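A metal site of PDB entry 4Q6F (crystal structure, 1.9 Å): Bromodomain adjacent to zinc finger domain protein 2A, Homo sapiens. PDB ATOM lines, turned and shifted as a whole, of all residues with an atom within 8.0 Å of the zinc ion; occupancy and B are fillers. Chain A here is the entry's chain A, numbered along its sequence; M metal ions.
The side-chain sulfur of Cys 27 sits close to the guanidinium group of Arg 29 (3.3 Å). The side-chain sulfur (SG) of Cys 24 lies close to the backbone NH (N) of Gly 26 (3.2 Å). The backbone carbonyl oxygen of Gly 26 sits close to the side-chain sulfur of Cys 53 (3.7 Å). The backbone NH of Val 52 lies close to the side-chain sulfur of Cys 50 (3.4 Å). O of Arg 29 sits at hydrogen-bond distance from N of Cys 24, 2.9 Å away.
The nearest printed residue that does not touch the zinc ion is Gly 26 (4.1 Å).
The zinc ion is bound by the side-chain sulfur (SG) of Cys 27 (2.2 Å), the side-chain sulfur (SG) of Cys 24 (2.2 Å), the side-chain sulfur (SG) of Cys 50 (2.3 Å) and the side-chain sulfur (SG) of Cys 53 (2.4 Å).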
ATOM      1  N   LEU A  10     -13.513 -26.175 -16.903  1.00  0.00           N
ATOM      2  CA  LEU A  10     -13.913 -26.688 -18.202  1.00  0.00           C
ATOM      3  C   LEU A  10     -15.131 -27.583 -18.131  1.00  0.00           C
ATOM      4  O   LEU A  10     -15.880 -27.672 -19.090  1.00  0.00           O
ATOM      5  CB  LEU A  10     -12.783 -27.513 -18.855  1.00  0.00           C
ATOM      6  CG  LEU A  10     -11.691 -26.733 -19.576  1.00  0.00           C
ATOM      7  CD1 LEU A  10     -10.509 -27.641 -19.888  1.00  0.00           C
ATOM      8  CD2 LEU A  10     -12.241 -26.082 -20.847  1.00  0.00           C
ATOM      9  N   LEU A  23      -5.341 -24.974 -12.464  1.00  0.00           N
ATOM     10  CA  LEU A  23      -5.006 -24.151 -13.615  1.00  0.00           C
ATOM     11  C   LEU A  23      -4.081 -24.936 -14.595  1.00  0.00           C
ATOM     12  O   LEU A  23      -3.108 -25.582 -14.162  1.00  0.00           O
ATOM     13  CB  LEU A  23      -4.292 -22.909 -13.154  1.00  0.00           C
ATOM     14  CG  LEU A  23      -4.945 -21.949 -12.148  1.00  0.00           C
ATOM     15  CD1 LEU A  23      -4.039 -20.731 -11.943  1.00  0.00           C
ATOM     16  CD2 LEU A  23      -6.321 -21.503 -12.626  1.00  0.00           C
ATOM     17  N   CYS A  24      -4.401 -24.878 -15.901  1.00  0.00           N
ATOM     18  CA  CYS A  24      -3.537 -25.468 -16.918  1.00  0.00           C
ATOM     19  C   CYS A  24      -2.208 -24.720 -16.952  1.00  0.00           C
ATOM     20  O   CYS A  24      -2.189 -23.464 -16.898  1.00  0.00           O
ATOM     21  CB  CYS A  24      -4.214 -25.431 -18.304  1.00  0.00           C
ATOM     22  SG  CYS A  24      -3.259 -26.244 -19.599  1.00  0.00           S
ATOM     23  N   ASP A  25      -1.102 -25.474 -16.999  1.00  0.00           N
ATOM     24  CA  ASP A  25       0.223 -24.883 -17.204  1.00  0.00           C
ATOM     25  C   ASP A  25       0.505 -24.479 -18.665  1.00  0.00           C
ATOM     26  O   ASP A  25       1.482 -23.798 -18.920  1.00  0.00           O
ATOM     27  CB  ASP A  25       1.317 -25.810 -16.665  1.00  0.00           C
ATOM     28  CG  ASP A  25       1.338 -25.849 -15.141  1.00  0.00           C
ATOM     29  OD1 ASP A  25       1.541 -24.778 -14.536  1.00  0.00           O
ATOM     30  OD2 ASP A  25       1.106 -26.920 -14.560  1.00  0.00           O
ATOM     31  N   GLY A  26      -0.352 -24.855 -19.627  1.00  0.00           N
ATOM     32  CA  GLY A  26      -0.159 -24.479 -21.026  1.00  0.00           C
ATOM     33  C   GLY A  26      -1.075 -23.393 -21.578  1.00  0.00           C
ATOM     34  O   GLY A  26      -0.865 -22.934 -22.684  1.00  0.00           O
ATOM     35  N   CYS A  27      -2.118 -23.018 -20.837  1.00  0.00           N
ATOM     36  CA  CYS A  27      -3.082 -22.052 -21.328  1.00  0.00           C
ATOM     37  C   CYS A  27      -3.811 -21.419 -20.150  1.00  0.00           C
ATOM     38  O   CYS A  27      -3.418 -21.609 -19.003  1.00  0.00           O
ATOM     39  CB  CYS A  27      -4.057 -22.690 -22.322  1.00  0.00           C
ATOM     40  SG  CYS A  27      -5.275 -23.841 -21.577  1.00  0.00           S
ATOM     41  N   ASP A  28      -4.881 -20.685 -20.440  1.00  0.00           N
ATOM     42  CA  ASP A  28      -5.736 -20.042 -19.419  1.00  0.00           C
ATOM     43  C   ASP A  28      -6.902 -20.872 -18.887  1.00  0.00           C
ATOM     44  O   ASP A  28      -7.764 -20.324 -18.188  1.00  0.00           O
ATOM     45  CB  ASP A  28      -6.304 -18.742 -20.006  1.00  0.00           C
ATOM     46  CG  ASP A  28      -5.236 -17.705 -20.259  1.00  0.00           C
ATOM     47  OD1 ASP A  28      -4.120 -17.826 -19.674  1.00  0.00           O
ATOM     48  OD2 ASP A  28      -5.505 -16.758 -21.034  1.00  0.00           O
ATOM     49  N   ARG A  29      -6.974 -22.168 -19.197  1.00  0.00           N
ATOM     50  CA  ARG A  29      -8.129 -22.976 -18.788  1.00  0.00           C
ATOM     51  C   ARG A  29      -7.923 -23.562 -17.409  1.00  0.00           C
ATOM     52  O   ARG A  29      -6.818 -23.519 -16.852  1.00  0.00           O
ATOM     53  CB  ARG A  29      -8.389 -24.068 -19.813  1.00  0.00           C
ATOM     54  CG  ARG A  29      -8.706 -23.494 -21.192  1.00  0.00           C
ATOM     55  CD  ARG A  29      -8.839 -24.564 -22.240  1.00  0.00           C
ATOM     56  NE  ARG A  29      -9.281 -24.025 -23.525  1.00  0.00           N
ATOM     57  CZ  ARG A  29      -8.477 -23.485 -24.438  1.00  0.00           C
ATOM     58  NH1 ARG A  29      -7.163 -23.413 -24.219  1.00  0.00           N
ATOM     59  NH2 ARG A  29      -8.963 -23.034 -25.579  1.00  0.00           N
ATOM     60  N   GLY A  30      -8.994 -24.129 -16.864  1.00  0.00           N
ATOM     61  CA  GLY A  30      -8.958 -24.773 -15.549  1.00  0.00           C
ATOM     62  C   GLY A  30      -9.929 -25.919 -15.388  1.00  0.00           C
ATOM     63  O   GLY A  30     -10.751 -26.228 -16.271  1.00  0.00           O
ATOM     64  N   TRP A  48       0.478 -29.618 -15.029  1.00  0.00           N
ATOM     65  CA  TRP A  48      -0.771 -30.181 -15.497  1.00  0.00           C
ATOM     66  C   TRP A  48      -1.221 -29.462 -16.754  1.00  0.00           C
ATOM     67  O   TRP A  48      -1.274 -28.260 -16.796  1.00  0.00           O
ATOM     68  CB  TRP A  48      -1.874 -30.040 -14.432  1.00  0.00           C
ATOM     69  CG  TRP A  48      -3.140 -30.666 -14.909  1.00  0.00           C
ATOM     70  CD1 TRP A  48      -3.388 -32.001 -15.041  1.00  0.00           C
ATOM     71  CD2 TRP A  48      -4.319 -29.998 -15.377  1.00  0.00           C
ATOM     72  NE1 TRP A  48      -4.641 -32.209 -15.531  1.00  0.00           N
ATOM     73  CE2 TRP A  48      -5.234 -31.003 -15.748  1.00  0.00           C
ATOM     74  CE3 TRP A  48      -4.677 -28.661 -15.526  1.00  0.00           C
ATOM     75  CZ2 TRP A  48      -6.499 -30.698 -16.267  1.00  0.00           C
ATOM     76  CZ3 TRP A  48      -5.928 -28.360 -16.026  1.00  0.00           C
ATOM     77  CH2 TRP A  48      -6.839 -29.378 -16.396  1.00  0.00           C
ATOM     78  N   PHE A  49      -1.565 -30.240 -17.769  1.00  0.00           N
ATOM     79  CA  PHE A  49      -2.047 -29.746 -19.041  1.00  0.00           C
ATOM     80  C   PHE A  49      -3.446 -30.225 -19.311  1.00  0.00           C
ATOM     81  O   PHE A  49      -3.741 -31.414 -19.209  1.00  0.00           O
ATOM     82  CB  PHE A  49      -1.119 -30.264 -20.155  1.00  0.00           C
ATOM     83  CG  PHE A  49       0.262 -29.698 -20.037  1.00  0.00           C
ATOM     84  CD1 PHE A  49       0.493 -28.384 -20.422  1.00  0.00           C
ATOM     85  CD2 PHE A  49       1.294 -30.444 -19.492  1.00  0.00           C
ATOM     86  CE1 PHE A  49       1.772 -27.828 -20.307  1.00  0.00           C
ATOM     87  CE2 PHE A  49       2.574 -29.879 -19.356  1.00  0.00           C
ATOM     88  CZ  PHE A  49       2.807 -28.587 -19.761  1.00  0.00           C
ATOM     89  N   CYS A  50      -4.287 -29.271 -19.673  1.00  0.00           N
ATOM     90  CA  CYS A  50      -5.662 -29.528 -20.069  1.00  0.00           C
ATOM     91  C   CYS A  50      -5.767 -30.298 -21.397  1.00  0.00           C
ATOM     92  O   CYS A  50      -4.778 -30.510 -22.097  1.00  0.00           O
ATOM     93  CB  CYS A  50      -6.406 -28.188 -20.154  1.00  0.00           C
ATOM     94  SG  CYS A  50      -6.236 -27.267 -21.704  1.00  0.00           S
ATOM     95  N   THR A  51      -6.981 -30.727 -21.739  1.00  0.00           N
ATOM     96  CA  THR A  51      -7.250 -31.483 -22.942  1.00  0.00           C
ATOM     97  C   THR A  51      -6.964 -30.704 -24.243  1.00  0.00           C
ATOM     98  O   THR A  51      -6.511 -31.262 -25.258  1.00  0.00           O
ATOM     99  CB  THR A  51      -8.698 -32.026 -22.890  1.00  0.00           C
ATOM    100  OG1 THR A  51      -9.586 -30.968 -22.596  1.00  0.00           O
ATOM    101  CG2 THR A  51      -8.820 -33.016 -21.756  1.00  0.00           C
ATOM    102  N   VAL A  52      -7.137 -29.392 -24.212  1.00  0.00           N
ATOM    103  CA  VAL A  52      -6.800 -28.576 -25.356  1.00  0.00           C
ATOM    104  C   VAL A  52      -5.282 -28.543 -25.578  1.00  0.00           C
ATOM    105  O   VAL A  52      -4.763 -28.673 -26.741  1.00  0.00           O
ATOM    106  CB  VAL A  52      -7.387 -27.166 -25.219  1.00  0.00           C
ATOM    107  CG1 VAL A  52      -7.062 -26.340 -26.447  1.00  0.00           C
ATOM    108  CG2 VAL A  52      -8.884 -27.237 -24.983  1.00  0.00           C
ATOM    109  N   CYS A  53      -4.536 -28.409 -24.478  1.00  0.00           N
ATOM    110  CA  CYS A  53      -3.080 -28.375 -24.608  1.00  0.00           C
ATOM    111  C   CYS A  53      -2.531 -29.727 -25.028  1.00  0.00           C
ATOM    112  O   CYS A  53      -1.650 -29.794 -25.908  1.00  0.00           O
ATOM    113  CB  CYS A  53      -2.405 -27.862 -23.347  1.00  0.00           C
ATOM    114  SG  CYS A  53      -2.727 -26.110 -23.170  1.00  0.00           S
ATOM    115  N   LEU A  54      -3.062 -30.811 -24.456  1.00  0.00           N
ATOM    116  CA  LEU A  54      -2.663 -32.149 -24.895  1.00  0.00           C
ATOM    117  C   LEU A  54      -2.804 -32.371 -26.379  1.00  0.00           C
ATOM    118  O   LEU A  54      -1.939 -33.011 -26.982  1.00  0.00           O
ATOM    119  CB  LEU A  54      -3.457 -33.251 -24.221  1.00  0.00           C
ATOM    120  CG  LEU A  54      -3.115 -33.447 -22.755  1.00  0.00           C
ATOM    121  CD1 LEU A  54      -4.020 -34.549 -22.225  1.00  0.00           C
ATOM    122  CD2 LEU A  54      -1.671 -33.815 -22.495  1.00  0.00           C
HETATM  123 ZN    ZN M   1      -4.401 -25.855 -21.483  1.00  0.00          ZN
